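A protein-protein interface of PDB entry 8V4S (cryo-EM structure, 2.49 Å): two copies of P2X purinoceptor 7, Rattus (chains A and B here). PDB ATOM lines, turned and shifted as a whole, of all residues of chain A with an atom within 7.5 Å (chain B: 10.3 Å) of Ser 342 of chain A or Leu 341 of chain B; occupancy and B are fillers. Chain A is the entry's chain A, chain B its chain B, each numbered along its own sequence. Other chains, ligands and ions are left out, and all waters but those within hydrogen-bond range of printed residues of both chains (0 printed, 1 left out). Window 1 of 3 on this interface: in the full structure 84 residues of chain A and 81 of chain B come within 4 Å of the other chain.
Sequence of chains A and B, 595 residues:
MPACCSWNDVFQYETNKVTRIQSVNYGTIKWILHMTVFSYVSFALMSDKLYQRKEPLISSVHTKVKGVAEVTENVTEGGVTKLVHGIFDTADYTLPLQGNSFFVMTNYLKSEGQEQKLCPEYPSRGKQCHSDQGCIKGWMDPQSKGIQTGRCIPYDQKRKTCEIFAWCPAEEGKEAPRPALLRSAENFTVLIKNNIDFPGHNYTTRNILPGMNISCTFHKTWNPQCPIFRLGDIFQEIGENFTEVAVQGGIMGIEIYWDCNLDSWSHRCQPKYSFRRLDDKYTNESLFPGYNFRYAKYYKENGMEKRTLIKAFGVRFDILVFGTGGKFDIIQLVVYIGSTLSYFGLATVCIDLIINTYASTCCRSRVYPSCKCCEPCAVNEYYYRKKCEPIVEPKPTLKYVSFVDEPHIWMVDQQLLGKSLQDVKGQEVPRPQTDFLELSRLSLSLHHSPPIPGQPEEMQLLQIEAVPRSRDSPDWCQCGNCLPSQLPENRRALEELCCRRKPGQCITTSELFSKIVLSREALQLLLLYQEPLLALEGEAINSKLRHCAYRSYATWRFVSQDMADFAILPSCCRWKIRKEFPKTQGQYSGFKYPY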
ATOM      1  N   VAL A  37     -15.543  13.153  10.978  1.00  0.00           N
ATOM      2  CA  VAL A  37     -15.725  13.631  12.345  1.00  0.00           C
ATOM      3  C   VAL A  37     -16.911  12.935  13.002  1.00  0.00           C
ATOM      4  O   VAL A  37     -16.830  12.498  14.156  1.00  0.00           O
ATOM      5  CB  VAL A  37     -15.883  15.163  12.363  1.00  0.00           C
ATOM      6  CG1 VAL A  37     -16.310  15.639  13.741  1.00  0.00           C
ATOM      7  CG2 VAL A  37     -14.581  15.827  11.959  1.00  0.00           C
ATOM      8  N   ILE A 337     -21.541  15.442  23.960  1.00  0.00           N
ATOM      9  CA  ILE A 337     -21.909  16.063  22.692  1.00  0.00           C
ATOM     10  C   ILE A 337     -21.399  17.498  22.634  1.00  0.00           C
ATOM     11  O   ILE A 337     -20.896  17.952  21.599  1.00  0.00           O
ATOM     12  CB  ILE A 337     -23.432  15.981  22.479  1.00  0.00           C
ATOM     13  CG1 ILE A 337     -23.848  14.532  22.211  1.00  0.00           C
ATOM     14  CG2 ILE A 337     -23.869  16.872  21.327  1.00  0.00           C
ATOM     15  CD1 ILE A 337     -25.335  14.344  22.038  1.00  0.00           C
ATOM     16  N   GLY A 338     -21.517  18.231  23.741  1.00  0.00           N
ATOM     17  CA  GLY A 338     -20.974  19.577  23.778  1.00  0.00           C
ATOM     18  C   GLY A 338     -19.467  19.602  23.612  1.00  0.00           C
ATOM     19  O   GLY A 338     -18.914  20.527  23.011  1.00  0.00           O
ATOM     20  N   SER A 339     -18.781  18.593  24.150  1.00  0.00           N
ATOM     21  CA  SER A 339     -17.336  18.504  23.973  1.00  0.00           C
ATOM     22  C   SER A 339     -16.971  18.232  22.521  1.00  0.00           C
ATOM     23  O   SER A 339     -15.957  18.733  22.026  1.00  0.00           O
ATOM     24  CB  SER A 339     -16.760  17.420  24.881  1.00  0.00           C
ATOM     25  OG  SER A 339     -17.028  17.703  26.241  1.00  0.00           O
ATOM     26  N   THR A 340     -17.771  17.431  21.824  1.00  0.00           N
ATOM     27  CA  THR A 340     -17.445  17.077  20.446  1.00  0.00           C
ATOM     28  C   THR A 340     -18.005  18.048  19.410  1.00  0.00           C
ATOM     29  O   THR A 340     -17.677  17.914  18.228  1.00  0.00           O
ATOM     30  CB  THR A 340     -17.941  15.662  20.130  1.00  0.00           C
ATOM     31  OG1 THR A 340     -19.364  15.600  20.280  1.00  0.00           O
ATOM     32  CG2 THR A 340     -17.295  14.659  21.060  1.00  0.00           C
ATOM     33  N   LEU A 341     -18.837  19.011  19.815  1.00  0.00           N
ATOM     34  CA  LEU A 341     -19.484  19.891  18.842  1.00  0.00           C
ATOM     35  C   LEU A 341     -18.478  20.729  18.058  1.00  0.00           C
ATOM     36  O   LEU A 341     -18.650  20.942  16.852  1.00  0.00           O
ATOM     37  CB  LEU A 341     -20.498  20.793  19.542  1.00  0.00           C
ATOM     38  CG  LEU A 341     -21.922  20.248  19.666  1.00  0.00           C
ATOM     39  CD1 LEU A 341     -22.811  21.222  20.419  1.00  0.00           C
ATOM     40  CD2 LEU A 341     -22.501  19.927  18.298  1.00  0.00           C
ATOM     41  N   SER A 342     -17.432  21.229  18.719  1.00  0.00           N
ATOM     42  CA  SER A 342     -16.477  22.109  18.054  1.00  0.00           C
ATOM     43  C   SER A 342     -15.664  21.412  16.970  1.00  0.00           C
ATOM     44  O   SER A 342     -15.025  22.098  16.167  1.00  0.00           O
ATOM     45  CB  SER A 342     -15.522  22.731  19.074  1.00  0.00           C
ATOM     46  OG  SER A 342     -16.167  23.722  19.850  1.00  0.00           O
ATOM     47  N   TYR A 343     -15.661  20.081  16.927  1.00  0.00           N
ATOM     48  CA  TYR A 343     -14.897  19.361  15.917  1.00  0.00           C
ATOM     49  C   TYR A 343     -15.533  19.418  14.537  1.00  0.00           C
ATOM     50  O   TYR A 343     -14.882  19.036  13.560  1.00  0.00           O
ATOM     51  CB  TYR A 343     -14.717  17.901  16.333  1.00  0.00           C
ATOM     52  CG  TYR A 343     -13.613  17.688  17.337  1.00  0.00           C
ATOM     53  CD1 TYR A 343     -12.299  18.003  17.029  1.00  0.00           C
ATOM     54  CD2 TYR A 343     -13.884  17.168  18.594  1.00  0.00           C
ATOM     55  CE1 TYR A 343     -11.288  17.811  17.944  1.00  0.00           C
ATOM     56  CE2 TYR A 343     -12.880  16.971  19.513  1.00  0.00           C
ATOM     57  CZ  TYR A 343     -11.583  17.293  19.184  1.00  0.00           C
ATOM     58  OH  TYR A 343     -10.578  17.098  20.097  1.00  0.00           O
ATOM     59  N   PHE A 344     -16.773  19.886  14.429  1.00  0.00           N
ATOM     60  CA  PHE A 344     -17.443  20.000  13.143  1.00  0.00           C
ATOM     61  C   PHE A 344     -17.095  21.288  12.409  1.00  0.00           C
ATOM     62  O   PHE A 344     -17.601  21.510  11.305  1.00  0.00           O
ATOM     63  CB  PHE A 344     -18.956  19.885  13.329  1.00  0.00           C
ATOM     64  CG  PHE A 344     -19.419  18.489  13.633  1.00  0.00           C
ATOM     65  CD1 PHE A 344     -19.544  17.551  12.620  1.00  0.00           C
ATOM     66  CD2 PHE A 344     -19.716  18.109  14.931  1.00  0.00           C
ATOM     67  CE1 PHE A 344     -19.966  16.265  12.895  1.00  0.00           C
ATOM     68  CE2 PHE A 344     -20.137  16.823  15.211  1.00  0.00           C
ATOM     69  CZ  PHE A 344     -20.263  15.900  14.192  1.00  0.00           C
ATOM     70  N   GLY A 345     -16.254  22.136  12.991  1.00  0.00           N
ATOM     71  CA  GLY A 345     -15.647  23.244  12.293  1.00  0.00           C
ATOM     72  C   GLY A 345     -14.376  22.882  11.559  1.00  0.00           C
ATOM     73  O   GLY A 345     -13.713  23.765  11.005  1.00  0.00           O
ATOM     74  N   LEU A 346     -14.020  21.595  11.548  1.00  0.00           N
ATOM     75  CA  LEU A 346     -12.802  21.155  10.875  1.00  0.00           C
ATOM     76  C   LEU A 346     -12.871  21.406   9.375  1.00  0.00           C
ATOM     77  O   LEU A 346     -11.882  21.827   8.766  1.00  0.00           O
ATOM     78  CB  LEU A 346     -12.561  19.671  11.154  1.00  0.00           C
ATOM     79  CG  LEU A 346     -11.255  19.080  10.619  1.00  0.00           C
ATOM     80  CD1 LEU A 346     -10.089  19.464  11.512  1.00  0.00           C
ATOM     81  CD2 LEU A 346     -11.359  17.571  10.477  1.00  0.00           C
ATOM     82  N   VAL A 349     -12.348  25.091   8.768  1.00  0.00           N
ATOM     83  CA  VAL A 349     -10.953  25.471   8.984  1.00  0.00           C
ATOM     84  C   VAL A 349     -10.091  25.027   7.808  1.00  0.00           C
ATOM     85  O   VAL A 349      -9.294  25.806   7.272  1.00  0.00           O
ATOM     86  CB  VAL A 349     -10.441  24.891  10.315  1.00  0.00           C
ATOM     87  CG1 VAL A 349      -8.927  24.972  10.388  1.00  0.00           C
ATOM     88  CG2 VAL A 349     -11.067  25.626  11.483  1.00  0.00           C
ATOM     89  N   HIS B  34      -4.998  34.833  22.560  1.00  0.00           N
ATOM     90  CA  HIS B  34      -4.754  33.481  22.066  1.00  0.00           C
ATOM     91  C   HIS B  34      -3.658  32.792  22.866  1.00  0.00           C
ATOM     92  O   HIS B  34      -3.791  31.619  23.232  1.00  0.00           O
ATOM     93  CB  HIS B  34      -4.378  33.522  20.586  1.00  0.00           C
ATOM     94  CG  HIS B  34      -5.552  33.612  19.662  1.00  0.00           C
ATOM     95  ND1 HIS B  34      -6.840  33.326  20.062  1.00  0.00           N
ATOM     96  CD2 HIS B  34      -5.634  33.959  18.357  1.00  0.00           C
ATOM     97  CE1 HIS B  34      -7.662  33.491  19.041  1.00  0.00           C
ATOM     98  NE2 HIS B  34      -6.955  33.875  17.994  1.00  0.00           N
ATOM     99  N   VAL B  37      -4.975  31.864  26.401  1.00  0.00           N
ATOM    100  CA  VAL B  37      -5.852  30.698  26.370  1.00  0.00           C
ATOM    101  C   VAL B  37      -5.047  29.429  26.122  1.00  0.00           C
ATOM    102  O   VAL B  37      -5.256  28.406  26.787  1.00  0.00           O
ATOM    103  CB  VAL B  37      -6.959  30.884  25.314  1.00  0.00           C
ATOM    104  CG1 VAL B  37      -7.723  29.589  25.108  1.00  0.00           C
ATOM    105  CG2 VAL B  37      -7.905  31.990  25.738  1.00  0.00           C
ATOM    106  N   PHE B  38      -4.113  29.473  25.170  1.00  0.00           N
ATOM    107  CA  PHE B  38      -3.297  28.297  24.877  1.00  0.00           C
ATOM    108  C   PHE B  38      -2.449  27.900  26.078  1.00  0.00           C
ATOM    109  O   PHE B  38      -2.328  26.709  26.391  1.00  0.00           O
ATOM    110  CB  PHE B  38      -2.411  28.563  23.659  1.00  0.00           C
ATOM    111  CG  PHE B  38      -1.566  27.389  23.262  1.00  0.00           C
ATOM    112  CD1 PHE B  38      -2.088  26.380  22.472  1.00  0.00           C
ATOM    113  CD2 PHE B  38      -0.251  27.290  23.683  1.00  0.00           C
ATOM    114  CE1 PHE B  38      -1.317  25.297  22.109  1.00  0.00           C
ATOM    115  CE2 PHE B  38       0.525  26.206  23.325  1.00  0.00           C
ATOM    116  CZ  PHE B  38      -0.009  25.210  22.537  1.00  0.00           C
ATOM    117  N   VAL B  41      -4.702  26.301  28.739  1.00  0.00           N
ATOM    118  CA  VAL B  41      -5.185  24.988  28.319  1.00  0.00           C
ATOM    119  C   VAL B  41      -4.071  23.954  28.406  1.00  0.00           C
ATOM    120  O   VAL B  41      -4.278  22.835  28.891  1.00  0.00           O
ATOM    121  CB  VAL B  41      -5.790  25.076  26.904  1.00  0.00           C
ATOM    122  CG1 VAL B  41      -5.878  23.702  26.265  1.00  0.00           C
ATOM    123  CG2 VAL B  41      -7.161  25.726  26.965  1.00  0.00           C
ATOM    124  N   SER B  42      -2.866  24.319  27.959  1.00  0.00           N
ATOM    125  CA  SER B  42      -1.729  23.408  28.057  1.00  0.00           C
ATOM    126  C   SER B  42      -1.374  23.114  29.509  1.00  0.00           C
ATOM    127  O   SER B  42      -1.064  21.968  29.858  1.00  0.00           O
ATOM    128  CB  SER B  42      -0.527  23.993  27.321  1.00  0.00           C
ATOM    129  OG  SER B  42      -0.832  24.223  25.958  1.00  0.00           O
ATOM    130  N   LEU B 333      -7.825  12.607  25.505  1.00  0.00           N
ATOM    131  CA  LEU B 333      -7.213  13.787  24.905  1.00  0.00           C
ATOM    132  C   LEU B 333      -8.163  14.467  23.928  1.00  0.00           C
ATOM    133  O   LEU B 333      -8.276  15.700  23.916  1.00  0.00           O
ATOM    134  CB  LEU B 333      -5.911  13.399  24.206  1.00  0.00           C
ATOM    135  CG  LEU B 333      -5.130  14.532  23.542  1.00  0.00           C
ATOM    136  CD1 LEU B 333      -4.588  15.498  24.581  1.00  0.00           C
ATOM    137  CD2 LEU B 333      -4.009  13.980  22.685  1.00  0.00           C
ATOM    138  N   VAL B 334      -8.858  13.681  23.102  1.00  0.00           N
ATOM    139  CA  VAL B 334      -9.787  14.257  22.135  1.00  0.00           C
ATOM    140  C   VAL B 334     -10.922  14.978  22.850  1.00  0.00           C
ATOM    141  O   VAL B 334     -11.311  16.087  22.464  1.00  0.00           O
ATOM    142  CB  VAL B 334     -10.313  13.164  21.183  1.00  0.00           C
ATOM    143  CG1 VAL B 334     -11.437  13.702  20.319  1.00  0.00           C
ATOM    144  CG2 VAL B 334      -9.187  12.639  20.312  1.00  0.00           C
ATOM    145  N   VAL B 335     -11.459  14.372  23.912  1.00  0.00           N
ATOM    146  CA  VAL B 335     -12.547  14.998  24.656  1.00  0.00           C
ATOM    147  C   VAL B 335     -12.079  16.292  25.311  1.00  0.00           C
ATOM    148  O   VAL B 335     -12.785  17.308  25.281  1.00  0.00           O
ATOM    149  CB  VAL B 335     -13.129  14.010  25.685  1.00  0.00           C
ATOM    150  CG1 VAL B 335     -14.019  14.729  26.680  1.00  0.00           C
ATOM    151  CG2 VAL B 335     -13.911  12.919  24.980  1.00  0.00           C
ATOM    152  N   TYR B 336     -10.883  16.287  25.908  1.00  0.00           N
ATOM    153  CA  TYR B 336     -10.380  17.503  26.543  1.00  0.00           C
ATOM    154  C   TYR B 336     -10.153  18.615  25.525  1.00  0.00           C
ATOM    155  O   TYR B 336     -10.487  19.781  25.778  1.00  0.00           O
ATOM    156  CB  TYR B 336      -9.090  17.212  27.310  1.00  0.00           C
ATOM    157  CG  TYR B 336      -8.445  18.466  27.851  1.00  0.00           C
ATOM    158  CD1 TYR B 336      -8.929  19.076  28.998  1.00  0.00           C
ATOM    159  CD2 TYR B 336      -7.371  19.058  27.197  1.00  0.00           C
ATOM    160  CE1 TYR B 336      -8.356  20.230  29.484  1.00  0.00           C
ATOM    161  CE2 TYR B 336      -6.796  20.212  27.677  1.00  0.00           C
ATOM    162  CZ  TYR B 336      -7.291  20.790  28.823  1.00  0.00           C
ATOM    163  OH  TYR B 336      -6.719  21.940  29.309  1.00  0.00           O
ATOM    164  N   ILE B 337      -9.571  18.280  24.372  1.00  0.00           N
ATOM    165  CA  ILE B 337      -9.318  19.293  23.351  1.00  0.00           C
ATOM    166  C   ILE B 337     -10.632  19.854  22.821  1.00  0.00           C
ATOM    167  O   ILE B 337     -10.764  21.066  22.608  1.00  0.00           O
ATOM    168  CB  ILE B 337      -8.442  18.709  22.226  1.00  0.00           C
ATOM    169  CG1 ILE B 337      -7.020  18.467  22.737  1.00  0.00           C
ATOM    170  CG2 ILE B 337      -8.415  19.638  21.022  1.00  0.00           C
ATOM    171  CD1 ILE B 337      -6.099  17.849  21.716  1.00  0.00           C
ATOM    172  N   GLY B 338     -11.621  18.988  22.604  1.00  0.00           N
ATOM    173  CA  GLY B 338     -12.924  19.470  22.181  1.00  0.00           C
ATOM    174  C   GLY B 338     -13.582  20.358  23.219  1.00  0.00           C
ATOM    175  O   GLY B 338     -14.289  21.309  22.878  1.00  0.00           O
ATOM    176  N   SER B 339     -13.369  20.052  24.500  1.00  0.00           N
ATOM    177  CA  SER B 339     -13.906  20.898  25.560  1.00  0.00           C
ATOM    178  C   SER B 339     -13.235  22.264  25.574  1.00  0.00           C
ATOM    179  O   SER B 339     -13.881  23.276  25.862  1.00  0.00           O
ATOM    180  CB  SER B 339     -13.746  20.210  26.913  1.00  0.00           C
ATOM    181  OG  SER B 339     -14.431  18.973  26.938  1.00  0.00           O
ATOM    182  N   THR B 340     -11.940  22.317  25.280  1.00  0.00           N
ATOM    183  CA  THR B 340     -11.221  23.586  25.337  1.00  0.00           C
ATOM    184  C   THR B 340     -11.245  24.369  24.027  1.00  0.00           C
ATOM    185  O   THR B 340     -10.781  25.512  24.006  1.00  0.00           O
ATOM    186  CB  THR B 340      -9.766  23.352  25.756  1.00  0.00           C
ATOM    187  OG1 THR B 340      -9.111  22.513  24.797  1.00  0.00           O
ATOM    188  CG2 THR B 340      -9.709  22.695  27.118  1.00  0.00           C
ATOM    189  N   LEU B 341     -11.767  23.791  22.943  1.00  0.00           N
ATOM    190  CA  LEU B 341     -11.709  24.461  21.644  1.00  0.00           C
ATOM    191  C   LEU B 341     -12.483  25.777  21.634  1.00  0.00           C
ATOM    192  O   LEU B 341     -12.037  26.757  21.027  1.00  0.00           O
ATOM    193  CB  LEU B 341     -12.227  23.531  20.549  1.00  0.00           C
ATOM    194  CG  LEU B 341     -11.190  22.626  19.879  1.00  0.00           C
ATOM    195  CD1 LEU B 341     -11.846  21.725  18.847  1.00  0.00           C
ATOM    196  CD2 LEU B 341     -10.074  23.446  19.256  1.00  0.00           C
ATOM    197  N   SER B 342     -13.649  25.821  22.282  1.00  0.00           N
ATOM    198  CA  SER B 342     -14.483  27.018  22.245  1.00  0.00           C
ATOM    199  C   SER B 342     -13.859  28.213  22.955  1.00  0.00           C
ATOM    200  O   SER B 342     -14.335  29.336  22.765  1.00  0.00           O
ATOM    201  CB  SER B 342     -15.855  26.733  22.855  1.00  0.00           C
ATOM    202  OG  SER B 342     -16.649  25.936  21.997  1.00  0.00           O
ATOM    203  N   TYR B 343     -12.823  28.007  23.766  1.00  0.00           N
ATOM    204  CA  TYR B 343     -12.190  29.112  24.475  1.00  0.00           C
ATOM    205  C   TYR B 343     -11.331  29.984  23.574  1.00  0.00           C
ATOM    206  O   TYR B 343     -10.919  31.066  24.002  1.00  0.00           O
ATOM    207  CB  TYR B 343     -11.341  28.580  25.629  1.00  0.00           C
ATOM    208  CG  TYR B 343     -12.138  28.229  26.859  1.00  0.00           C
ATOM    209  CD1 TYR B 343     -12.866  29.197  27.537  1.00  0.00           C
ATOM    210  CD2 TYR B 343     -12.162  26.931  27.347  1.00  0.00           C
ATOM    211  CE1 TYR B 343     -13.595  28.880  28.661  1.00  0.00           C
ATOM    212  CE2 TYR B 343     -12.888  26.607  28.469  1.00  0.00           C
ATOM    213  CZ  TYR B 343     -13.602  27.584  29.124  1.00  0.00           C
ATOM    214  OH  TYR B 343     -14.327  27.266  30.244  1.00  0.00           O
ATOM    215  N   PHE B 344     -11.057  29.551  22.348  1.00  0.00           N
ATOM    216  CA  PHE B 344     -10.265  30.337  21.415  1.00  0.00           C
ATOM    217  C   PHE B 344     -11.094  31.367  20.660  1.00  0.00           C
ATOM    218  O   PHE B 344     -10.542  32.099  19.833  1.00  0.00           O
ATOM    219  CB  PHE B 344      -9.543  29.413  20.432  1.00  0.00           C
ATOM    220  CG  PHE B 344      -8.389  28.671  21.043  1.00  0.00           C
ATOM    221  CD1 PHE B 344      -7.170  29.300  21.238  1.00  0.00           C
ATOM    222  CD2 PHE B 344      -8.526  27.351  21.438  1.00  0.00           C
ATOM    223  CE1 PHE B 344      -6.106  28.624  21.801  1.00  0.00           C
ATOM    224  CE2 PHE B 344      -7.465  26.670  22.005  1.00  0.00           C
ATOM    225  CZ  PHE B 344      -6.254  27.308  22.187  1.00  0.00           C
ATOM    226  N   GLY B 345     -12.394  31.442  20.921  1.00  0.00           N
ATOM    227  CA  GLY B 345     -13.224  32.536  20.478  1.00  0.00           C
ATOM    228  C   GLY B 345     -13.226  33.720  21.418  1.00  0.00           C
ATOM    229  O   GLY B 345     -13.972  34.680  21.197  1.00  0.00           O
ATOM    230  N   LEU B 346     -12.404  33.670  22.469  1.00  0.00           N
ATOM    231  CA  LEU B 346     -12.349  34.762  23.437  1.00  0.00           C
ATOM    232  C   LEU B 346     -11.853  36.050  22.796  1.00  0.00           C
ATOM    233  O   LEU B 346     -12.375  37.132  23.082  1.00  0.00           O
ATOM    234  CB  LEU B 346     -11.449  34.372  24.610  1.00  0.00           C
ATOM    235  CG  LEU B 346     -11.379  35.362  25.774  1.00  0.00           C
ATOM    236  CD1 LEU B 346     -12.615  35.246  26.650  1.00  0.00           C
ATOM    237  CD2 LEU B 346     -10.113  35.156  26.588  1.00  0.00           C
ATOM    238  N   ALA B 347     -10.827  35.959  21.944  1.00  0.00           N
ATOM    239  CA  ALA B 347     -10.315  37.151  21.278  1.00  0.00           C
ATOM    240  C   ALA B 347     -11.375  37.777  20.384  1.00  0.00           C
ATOM    241  O   ALA B 347     -11.551  39.002  20.378  1.00  0.00           O
ATOM    242  CB  ALA B 347      -9.064  36.808  20.472  1.00  0.00           C
ATOM    243  N   THR B 348     -12.097  36.949  19.629  1.00  0.00           N
ATOM    244  CA  THR B 348     -13.175  37.455  18.789  1.00  0.00           C
ATOM    245  C   THR B 348     -14.243  38.138  19.630  1.00  0.00           C
ATOM    246  O   THR B 348     -14.683  39.246  19.313  1.00  0.00           O
ATOM    247  CB  THR B 348     -13.780  36.315  17.972  1.00  0.00           C
ATOM    248  OG1 THR B 348     -12.833  35.875  16.993  1.00  0.00           O
ATOM    249  CG2 THR B 348     -15.050  36.770  17.277  1.00  0.00           C
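The backbone carbonyl oxygen of Val 335 of chain B lies within hydrogen-bond range of the side-chain hydroxyl of Ser 339 of chain B (2.9 Å). O of Ile 337 of chain B sits at hydrogen-bond distance from OG1 of Thr 340 of chain B, at 3.1 Å.
Ser 339 of chain A touches Gly 338 of chain B, but with the chains exchanged Gly 338 of chain A does not touch Ser 339 of chain B (5.6 Å). Ser 342 of chain A touches Leu 341 of chain B, but with the chains exchanged Leu 341 of chain A does not touch Ser 342 of chain B (6.8 Å). Tyr 343 of chain A touches Ile 337 of chain B, but with the chains exchanged Ile 337 of chain A does not touch Tyr 343 of chain B (13.1 Å). Tyr 343 of chain A touches Gly 338 of chain B, but with the chains exchanged Gly 338 of chain A does not touch Tyr 343 of chain B (9.7 Å). Of the 8 pairs that touch across the chains among the printed residues, 2 have their exchanged pair printed and touching as well.
The side-chain hydroxyl of Tyr 343 of chain A lies within hydrogen-bond range of the backbone NH of Gly 338 of chain B, 3.3 Å away. The backbone carbonyl oxygen of Gly 338 of chain B lies close to the backbone carbonyl oxygen of Ser 339 of chain A, at 3.2 Å. OG of Ser 339 of chain B lies within hydrogen-bond range of OG of Ser 339 of chain A (3.0 Å). O of Val 334 of chain B lies within hydrogen-bond range of OH of Tyr 343 of chain A (2.7 Å). The side-chain hydroxyl (OG) of Ser 342 of chain B is in hydrogen-bond range of the side-chain hydroxyl (OG) of Ser 342 of chain A.
CB of Ser 339 of chain A touches O of Val 335 of chain B, at 3.997 Å. Ser 342 of chain A touches Leu 341 of chain B (CB to CB, 3.7 Å). Ile 337 of chain B touches Tyr 343 of chain A (CB to OH, 3.4 Å).
Gly 338 of chain A touches none of the printed residues of chain B. Printed residues of chain B within 4 Å of Ser 339 of chain A: Val 335, Gly 338 and Ser 339. Ser 342 of chain A touches two residues of chain B. Of chain B, only Val 334, Ile 337 and Gly 338 come within 4 Å of Tyr 343 of chain A. No residue of chain B comes within 4 Å of Gly 345 of chain A. Printed residues of chain A within 4 Å of Val 334 of chain B: Tyr 343 (2.7 Å). Printed residues of chain A within 4 Å of Val 335 of chain B: Ser 339. Thr 340 of chain B touches none of the printed residues of chain A. Of the printed residues of chain A, Leu 341 of chain B touches Ser 342 (3.7 Å). The nearest residue of chain A that does not touch Leu 341 of chain B is Tyr 343 of chain A (4.1 Å). The nearest printed residue of chain A that does not touch Val 334 of chain B is Ser 339 of chain A (5.4 Å).
Of the 12 printed residues of chain A, 3 touch a printed residue of chain B. Hydrophobic or aromatic side chains of chain A within 4 Å of the printed part of chain B: Tyr 343. Of the 21 printed residues of chain B, 7 touch a printed residue of chain A. Hydrophobic or aromatic side chains of chain B within 4 Å of the printed part of chain A: Val 334, Ile 337 and Leu 341. Among the printed residues, 8 pairs touch across the chains. Among the printed residues, no Asp or Glu carboxylate lies within 4 Å of a Lys or Arg side-chain nitrogen of the other chain.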
